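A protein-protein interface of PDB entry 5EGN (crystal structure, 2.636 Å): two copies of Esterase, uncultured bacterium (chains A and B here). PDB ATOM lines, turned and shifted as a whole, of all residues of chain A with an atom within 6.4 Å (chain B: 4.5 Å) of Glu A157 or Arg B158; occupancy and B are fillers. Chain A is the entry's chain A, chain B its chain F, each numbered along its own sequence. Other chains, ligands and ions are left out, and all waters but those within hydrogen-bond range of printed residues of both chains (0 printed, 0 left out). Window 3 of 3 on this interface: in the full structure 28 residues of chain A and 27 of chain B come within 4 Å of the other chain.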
ATOM      1  N   ALA A 152       7.200 -16.477   1.232  1.00  0.00           N
ATOM      2  CA  ALA A 152       7.992 -17.503   1.895  1.00  0.00           C
ATOM      3  C   ALA A 152       7.324 -18.864   1.747  1.00  0.00           C
ATOM      4  O   ALA A 152       7.988 -19.876   1.511  1.00  0.00           O
ATOM      5  CB  ALA A 152       8.188 -17.159   3.365  1.00  0.00           C
ATOM      6  N   ARG A 153       6.000 -18.874   1.876  1.00  0.00           N
ATOM      7  CA  ARG A 153       5.208 -20.086   1.721  1.00  0.00           C
ATOM      8  C   ARG A 153       5.359 -20.654   0.313  1.00  0.00           C
ATOM      9  O   ARG A 153       5.423 -21.869   0.125  1.00  0.00           O
ATOM     10  CB  ARG A 153       3.740 -19.794   2.028  1.00  0.00           C
ATOM     11  CG  ARG A 153       2.829 -21.006   2.053  1.00  0.00           C
ATOM     12  CD  ARG A 153       1.433 -20.580   2.466  1.00  0.00           C
ATOM     13  NE  ARG A 153       0.454 -21.656   2.354  1.00  0.00           N
ATOM     14  CZ  ARG A 153      -0.344 -22.040   3.346  1.00  0.00           C
ATOM     15  NH1 ARG A 153      -0.275 -21.436   4.526  1.00  0.00           N
ATOM     16  NH2 ARG A 153      -1.210 -23.027   3.161  1.00  0.00           N
ATOM     17  N   SER A 154       5.421 -19.763  -0.671  1.00  0.00           N
ATOM     18  CA  SER A 154       5.628 -20.167  -2.057  1.00  0.00           C
ATOM     19  C   SER A 154       7.044 -20.689  -2.266  1.00  0.00           C
ATOM     20  O   SER A 154       7.254 -21.638  -3.017  1.00  0.00           O
ATOM     21  CB  SER A 154       5.349 -19.002  -3.007  1.00  0.00           C
ATOM     22  OG  SER A 154       3.977 -18.646  -2.985  1.00  0.00           O
ATOM     23  N   LYS A 155       8.012 -20.066  -1.600  1.00  0.00           N
ATOM     24  CA  LYS A 155       9.394 -20.532  -1.650  1.00  0.00           C
ATOM     25  C   LYS A 155       9.513 -21.922  -1.039  1.00  0.00           C
ATOM     26  O   LYS A 155      10.385 -22.705  -1.415  1.00  0.00           O
ATOM     27  CB  LYS A 155      10.324 -19.561  -0.921  1.00  0.00           C
ATOM     28  CG  LYS A 155      10.453 -18.208  -1.587  1.00  0.00           C
ATOM     29  CD  LYS A 155      11.423 -17.317  -0.832  1.00  0.00           C
ATOM     30  CE  LYS A 155      11.522 -15.943  -1.474  1.00  0.00           C
ATOM     31  NZ  LYS A 155      12.511 -15.070  -0.786  1.00  0.00           N
ATOM     32  N   ARG A 156       8.629 -22.219  -0.093  1.00  0.00           N
ATOM     33  CA  ARG A 156       8.621 -23.515   0.571  1.00  0.00           C
ATOM     34  C   ARG A 156       7.961 -24.584  -0.294  1.00  0.00           C
ATOM     35  O   ARG A 156       8.564 -25.619  -0.579  1.00  0.00           O
ATOM     36  CB  ARG A 156       7.904 -23.420   1.921  1.00  0.00           C
ATOM     37  CG  ARG A 156       8.073 -24.645   2.808  1.00  0.00           C
ATOM     38  CD  ARG A 156       7.186 -24.562   4.041  1.00  0.00           C
ATOM     39  NE  ARG A 156       5.781 -24.819   3.732  1.00  0.00           N
ATOM     40  CZ  ARG A 156       4.762 -24.170   4.284  1.00  0.00           C
ATOM     41  NH1 ARG A 156       4.983 -23.210   5.174  1.00  0.00           N
ATOM     42  NH2 ARG A 156       3.518 -24.476   3.941  1.00  0.00           N
ATOM     43  N   GLU A 157       6.728 -24.326  -0.719  1.00  0.00           N
ATOM     44  CA  GLU A 157       5.927 -25.346  -1.387  1.00  0.00           C
ATOM     45  C   GLU A 157       6.063 -25.348  -2.913  1.00  0.00           C
ATOM     46  O   GLU A 157       5.904 -26.391  -3.545  1.00  0.00           O
ATOM     47  CB  GLU A 157       4.453 -25.185  -0.998  1.00  0.00           C
ATOM     48  CG  GLU A 157       4.184 -25.371   0.491  1.00  0.00           C
ATOM     49  CD  GLU A 157       2.713 -25.250   0.850  1.00  0.00           C
ATOM     50  OE1 GLU A 157       1.905 -24.923  -0.043  1.00  0.00           O
ATOM     51  OE2 GLU A 157       2.366 -25.485   2.027  1.00  0.00           O
ATOM     52  N   ARG A 158       6.354 -24.191  -3.505  1.00  0.00           N
ATOM     53  CA  ARG A 158       6.474 -24.094  -4.962  1.00  0.00           C
ATOM     54  C   ARG A 158       7.723 -23.331  -5.418  1.00  0.00           C
ATOM     55  O   ARG A 158       7.617 -22.207  -5.906  1.00  0.00           O
ATOM     56  CB  ARG A 158       5.229 -23.422  -5.557  1.00  0.00           C
ATOM     57  CG  ARG A 158       3.902 -23.974  -5.056  1.00  0.00           C
ATOM     58  CD  ARG A 158       2.736 -23.473  -5.894  1.00  0.00           C
ATOM     59  NE  ARG A 158       1.447 -23.852  -5.322  1.00  0.00           N
ATOM     60  CZ  ARG A 158       0.400 -24.259  -6.033  1.00  0.00           C
ATOM     61  NH1 ARG A 158       0.485 -24.350  -7.353  1.00  0.00           N
ATOM     62  NH2 ARG A 158      -0.733 -24.581  -5.424  1.00  0.00           N
ATOM     63  N   PRO A 159       8.911 -23.941  -5.267  1.00  0.00           N
ATOM     64  CA  PRO A 159      10.172 -23.316  -5.698  1.00  0.00           C
ATOM     65  C   PRO A 159      10.286 -23.191  -7.223  1.00  0.00           C
ATOM     66  O   PRO A 159      11.054 -22.365  -7.750  1.00  0.00           O
ATOM     67  CB  PRO A 159      11.239 -24.269  -5.148  1.00  0.00           C
ATOM     68  CG  PRO A 159      10.544 -25.583  -5.022  1.00  0.00           C
ATOM     69  CD  PRO A 159       9.134 -25.257  -4.641  1.00  0.00           C
ATOM     70  N   GLU A 160       9.506 -24.009  -7.924  1.00  0.00           N
ATOM     71  CA  GLU A 160       9.502 -24.022  -9.383  1.00  0.00           C
ATOM     72  C   GLU A 160       9.079 -22.677  -9.974  1.00  0.00           C
ATOM     73  O   GLU A 160       9.415 -22.361 -11.118  1.00  0.00           O
ATOM     74  CB  GLU A 160       8.582 -25.128  -9.902  1.00  0.00           C
ATOM     75  CG  GLU A 160       7.110 -24.939  -9.558  1.00  0.00           C
ATOM     76  CD  GLU A 160       6.702 -25.667  -8.293  1.00  0.00           C
ATOM     77  OE1 GLU A 160       7.594 -26.127  -7.550  1.00  0.00           O
ATOM     78  OE2 GLU A 160       5.484 -25.788  -8.046  1.00  0.00           O
ATOM     79  N   ARG A 248      -1.189 -19.378  -5.915  1.00  0.00           N
ATOM     80  CA  ARG A 248      -2.440 -20.016  -5.513  1.00  0.00           C
ATOM     81  C   ARG A 248      -3.460 -19.928  -6.647  1.00  0.00           C
ATOM     82  O   ARG A 248      -4.435 -19.185  -6.549  1.00  0.00           O
ATOM     83  CB  ARG A 248      -3.005 -19.371  -4.242  1.00  0.00           C
ATOM     84  CG  ARG A 248      -2.028 -19.319  -3.076  1.00  0.00           C
ATOM     85  CD  ARG A 248      -2.711 -18.894  -1.785  1.00  0.00           C
ATOM     86  NE  ARG A 248      -3.631 -19.916  -1.295  1.00  0.00           N
ATOM     87  CZ  ARG A 248      -3.260 -20.965  -0.568  1.00  0.00           C
ATOM     88  NH1 ARG A 248      -1.985 -21.135  -0.246  1.00  0.00           N
ATOM     89  NH2 ARG A 248      -4.164 -21.847  -0.164  1.00  0.00           N
ATOM     90  N   SER A 250      -5.983 -21.718  -8.133  1.00  0.00           N
ATOM     91  CA  SER A 250      -7.422 -21.944  -8.002  1.00  0.00           C
ATOM     92  C   SER A 250      -8.135 -20.784  -7.306  1.00  0.00           C
ATOM     93  O   SER A 250      -9.245 -20.408  -7.687  1.00  0.00           O
ATOM     94  CB  SER A 250      -7.692 -23.248  -7.249  1.00  0.00           C
ATOM     95  OG  SER A 250      -7.428 -24.374  -8.067  1.00  0.00           O
ATOM     96  N   ARG B 153      -2.431 -35.938  -2.601  1.00  0.00           N
ATOM     97  CA  ARG B 153      -1.764 -34.709  -2.193  1.00  0.00           C
ATOM     98  C   ARG B 153      -1.921 -33.623  -3.248  1.00  0.00           C
ATOM     99  O   ARG B 153      -2.069 -32.457  -2.913  1.00  0.00           O
ATOM    100  CB  ARG B 153      -0.278 -34.937  -1.922  1.00  0.00           C
ATOM    101  CG  ARG B 153       0.436 -33.670  -1.464  1.00  0.00           C
ATOM    102  CD  ARG B 153       1.946 -33.790  -1.557  1.00  0.00           C
ATOM    103  NE  ARG B 153       2.447 -34.952  -0.831  1.00  0.00           N
ATOM    104  CZ  ARG B 153       2.563 -35.015   0.491  1.00  0.00           C
ATOM    105  NH1 ARG B 153       2.208 -33.982   1.245  1.00  0.00           N
ATOM    106  NH2 ARG B 153       3.034 -36.114   1.063  1.00  0.00           N
ATOM    107  N   SER B 154      -1.882 -33.998  -4.520  1.00  0.00           N
ATOM    108  CA  SER B 154      -1.987 -33.003  -5.580  1.00  0.00           C
ATOM    109  C   SER B 154      -3.412 -32.485  -5.714  1.00  0.00           C
ATOM    110  O   SER B 154      -3.620 -31.302  -5.963  1.00  0.00           O
ATOM    111  CB  SER B 154      -1.506 -33.577  -6.909  1.00  0.00           C
ATOM    112  OG  SER B 154      -0.110 -33.795  -6.890  1.00  0.00           O
ATOM    113  N   ARG B 156      -5.328 -32.236  -3.286  1.00  0.00           N
ATOM    114  CA  ARG B 156      -5.497 -31.444  -2.070  1.00  0.00           C
ATOM    115  C   ARG B 156      -4.822 -30.074  -2.175  1.00  0.00           C
ATOM    116  O   ARG B 156      -5.475 -29.040  -2.034  1.00  0.00           O
ATOM    117  CB  ARG B 156      -4.945 -32.215  -0.866  1.00  0.00           C
ATOM    118  CG  ARG B 156      -5.297 -31.629   0.492  1.00  0.00           C
ATOM    119  CD  ARG B 156      -4.547 -32.357   1.603  1.00  0.00           C
ATOM    120  NE  ARG B 156      -4.481 -33.796   1.355  1.00  0.00           N
ATOM    121  CZ  ARG B 156      -3.375 -34.525   1.472  1.00  0.00           C
ATOM    122  NH1 ARG B 156      -3.408 -35.826   1.223  1.00  0.00           N
ATOM    123  NH2 ARG B 156      -2.236 -33.955   1.839  1.00  0.00           N
ATOM    124  N   GLU B 157      -3.519 -30.073  -2.434  1.00  0.00           N
ATOM    125  CA  GLU B 157      -2.710 -28.858  -2.410  1.00  0.00           C
ATOM    126  C   GLU B 157      -2.674 -28.117  -3.749  1.00  0.00           C
ATOM    127  O   GLU B 157      -2.437 -26.910  -3.783  1.00  0.00           O
ATOM    128  CB  GLU B 157      -1.279 -29.193  -1.973  1.00  0.00           C
ATOM    129  CG  GLU B 157      -1.192 -29.961  -0.660  1.00  0.00           C
ATOM    130  CD  GLU B 157       0.237 -30.264  -0.241  1.00  0.00           C
ATOM    131  OE1 GLU B 157       1.169 -29.898  -0.986  1.00  0.00           O
ATOM    132  OE2 GLU B 157       0.426 -30.871   0.833  1.00  0.00           O
ATOM    133  N   ARG B 158      -2.900 -28.833  -4.849  1.00  0.00           N
ATOM    134  CA  ARG B 158      -2.897 -28.214  -6.176  1.00  0.00           C
ATOM    135  C   ARG B 158      -4.108 -28.632  -7.019  1.00  0.00           C
ATOM    136  O   ARG B 158      -3.956 -29.352  -8.007  1.00  0.00           O
ATOM    137  CB  ARG B 158      -1.608 -28.566  -6.931  1.00  0.00           C
ATOM    138  CG  ARG B 158      -0.321 -28.346  -6.141  1.00  0.00           C
ATOM    139  CD  ARG B 158       0.915 -28.572  -7.006  1.00  0.00           C
ATOM    140  NE  ARG B 158       2.150 -28.531  -6.225  1.00  0.00           N
ATOM    141  CZ  ARG B 158       3.218 -27.802  -6.540  1.00  0.00           C
ATOM    142  NH1 ARG B 158       3.212 -27.042  -7.626  1.00  0.00           N
ATOM    143  NH2 ARG B 158       4.293 -27.831  -5.763  1.00  0.00           N
ATOM    144  N   PRO B 159      -5.315 -28.182  -6.635  1.00  0.00           N
ATOM    145  CA  PRO B 159      -6.544 -28.540  -7.359  1.00  0.00           C
ATOM    146  C   PRO B 159      -6.582 -27.977  -8.783  1.00  0.00           C
ATOM    147  O   PRO B 159      -7.326 -28.471  -9.645  1.00  0.00           O
ATOM    148  CB  PRO B 159      -7.649 -27.919  -6.499  1.00  0.00           C
ATOM    149  CG  PRO B 159      -6.981 -26.806  -5.773  1.00  0.00           C
ATOM    150  CD  PRO B 159      -5.590 -27.284  -5.500  1.00  0.00           C
ATOM    151  N   GLU B 160      -5.770 -26.951  -9.021  1.00  0.00           N
ATOM    152  CA  GLU B 160      -5.701 -26.299 -10.323  1.00  0.00           C
ATOM    153  C   GLU B 160      -5.230 -27.247 -11.424  1.00  0.00           C
ATOM    154  O   GLU B 160      -5.500 -27.018 -12.601  1.00  0.00           O
ATOM    155  CB  GLU B 160      -4.777 -25.080 -10.258  1.00  0.00           C
ATOM    156  CG  GLU B 160      -3.332 -25.392  -9.882  1.00  0.00           C
ATOM    157  CD  GLU B 160      -3.103 -25.409  -8.382  1.00  0.00           C
ATOM    158  OE1 GLU B 160      -4.094 -25.364  -7.625  1.00  0.00           O
ATOM    159  OE2 GLU B 160      -1.928 -25.461  -7.961  1.00  0.00           O
ATOM    160  N   ILE B 161      -4.524 -28.307 -11.042  1.00  0.00           N
ATOM    161  CA  ILE B 161      -4.032 -29.290 -12.004  1.00  0.00           C
ATOM    162  C   ILE B 161      -5.178 -30.118 -12.586  1.00  0.00           C
ATOM    163  O   ILE B 161      -5.329 -30.226 -13.807  1.00  0.00           O
ATOM    164  CB  ILE B 161      -2.990 -30.231 -11.362  1.00  0.00           C
ATOM    165  CG1 ILE B 161      -1.763 -29.437 -10.915  1.00  0.00           C
ATOM    166  CG2 ILE B 161      -2.588 -31.328 -12.335  1.00  0.00           C
ATOM    167  CD1 ILE B 161      -0.673 -30.289 -10.298  1.00  0.00           C
ATOM    168  N   LEU B 162      -5.986 -30.704 -11.708  1.00  0.00           N
ATOM    169  CA  LEU B 162      -7.158 -31.449 -12.147  1.00  0.00           C
ATOM    170  C   LEU B 162      -8.144 -30.518 -12.843  1.00  0.00           C
ATOM    171  O   LEU B 162      -8.805 -30.909 -13.807  1.00  0.00           O
ATOM    172  CB  LEU B 162      -7.836 -32.150 -10.971  1.00  0.00           C
ATOM    173  CG  LEU B 162      -9.076 -32.967 -11.342  1.00  0.00           C
ATOM    174  CD1 LEU B 162      -8.718 -34.054 -12.345  1.00  0.00           C
ATOM    175  CD2 LEU B 162      -9.731 -33.563 -10.107  1.00  0.00           C
ATOM    176  N   LEU B 246       4.002 -31.411 -13.337  1.00  0.00           N
ATOM    177  CA  LEU B 246       3.107 -30.409 -12.764  1.00  0.00           C
ATOM    178  C   LEU B 246       2.926 -30.589 -11.258  1.00  0.00           C
ATOM    179  O   LEU B 246       2.834 -29.610 -10.518  1.00  0.00           O
ATOM    180  CB  LEU B 246       1.740 -30.452 -13.446  1.00  0.00           C
ATOM    181  CG  LEU B 246       1.578 -29.715 -14.773  1.00  0.00           C
ATOM    182  CD1 LEU B 246       0.117 -29.728 -15.194  1.00  0.00           C
ATOM    183  CD2 LEU B 246       2.096 -28.291 -14.665  1.00  0.00           C
ATOM    184  N   GLU B 247       2.867 -31.839 -10.811  1.00  0.00           N
ATOM    185  CA  GLU B 247       2.593 -32.135  -9.408  1.00  0.00           C
ATOM    186  C   GLU B 247       3.785 -31.796  -8.515  1.00  0.00           C
ATOM    187  O   GLU B 247       3.618 -31.230  -7.436  1.00  0.00           O
ATOM    188  CB  GLU B 247       2.195 -33.603  -9.245  1.00  0.00           C
ATOM    189  CG  GLU B 247       0.899 -33.964  -9.965  1.00  0.00           C
ATOM    190  CD  GLU B 247       0.474 -35.398  -9.730  1.00  0.00           C
ATOM    191  OE1 GLU B 247       0.375 -35.805  -8.554  1.00  0.00           O
ATOM    192  OE2 GLU B 247       0.233 -36.120 -10.721  1.00  0.00           O
ATOM    193  N   PRO B 249       7.024 -30.113  -9.914  1.00  0.00           N
ATOM    194  CA  PRO B 249       7.805 -29.614 -11.055  1.00  0.00           C
ATOM    195  C   PRO B 249       9.309 -29.510 -10.802  1.00  0.00           C
ATOM    196  O   PRO B 249      10.090 -29.926 -11.656  1.00  0.00           O
ATOM    197  CB  PRO B 249       7.212 -28.223 -11.298  1.00  0.00           C
ATOM    198  CG  PRO B 249       5.843 -28.291 -10.733  1.00  0.00           C
ATOM    199  CD  PRO B 249       5.967 -29.165  -9.526  1.00  0.00           C
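The backbone carbonyl oxygen of Glu A157 is in hydrogen-bond range of the guanidinium group of Arg B158, at 3.1 Å.
The backbone carbonyl oxygen (O) of Glu B157 lies within hydrogen-bond range of the guanidinium group (NH2) of Arg A158 (3.3 Å).
OE2 of Glu B160 lies within salt-bridge range of NH1 of Arg A158 (2.7 Å).
The side-chain carboxylate (OE2) of Glu A160 lies within salt-bridge range of the guanidinium group (NH1) of Arg B158 (2.6 Å).
OG of Ser A250 is in hydrogen-bond range of N of Glu B160.
The guanidinium group (NH2) of Arg A156 is in salt-bridge range of the side-chain carboxylate (OE2) of Glu A157, 2.5 Å away.
The guanidinium group (NH1) of Arg B153 lies within salt-bridge range of the side-chain carboxylate (OE2) of Glu B157 (3.6 Å).
The guanidinium group (NE) of Arg B158 sits at hydrogen-bond distance from the backbone carbonyl oxygen (O) of Glu B247.
Arg A158 touches Arg B158.
Pro B249 touches Glu A160 (CB to CB, 3.7 Å).
Ser A250 touches Pro B159.
Glu A157 touches just one residue of chain B: Arg B158.
Of the printed residues of chain B, Glu A160 touches Arg B158 and Pro B249.
Arg B156 touches none of the printed residues of chain A.
Of the printed residues of chain A, Glu B157 touches Arg A158.
Of chain A, only Glu A157, Arg A158 and Glu A160 come within 4 Å of Arg B158.
Of the printed residues of chain A, Pro B159 touches Ser A250.
Of the printed residues of chain A, Glu B160 touches Arg A158 and Ser A250.
Of the printed residues of chain A, Pro B249 touches Glu A160.
The nearest printed residue of chain A that does not touch Pro B159 is Arg A158 (5.6 Å).
Printed residues of chain B that touch a printed residue of chain A: Glu B157, Arg B158, Pro B159, Glu B160 and Pro B249.
Hydrophobic or aromatic side chains of chain B within 4 Å of the printed part of chain A: Pro B159 and Pro B249.
Among the printed residues, 8 pairs touch across the chains.
Among the printed residues, Asp or Glu carboxylates within 4 Å of a Lys or Arg side-chain nitrogen of the other chain: Arg A158 with Glu B160 and Glu A160 with Arg B158.
Glu A157 touches Arg B158, and with the chains exchanged Arg A158 touches Glu B157.
Arg B158 touches its own counterpart, Arg A158.
Arg A158 touches Glu B160, and with the chains exchanged Glu A160 touches Arg B158.
Positions printed for both chains: 153, 154, 156, 157, 158, 159 and 160.
Of the 8 pairs that touch across the chains among the printed residues, 5 have their exchanged pair printed and touching as well.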
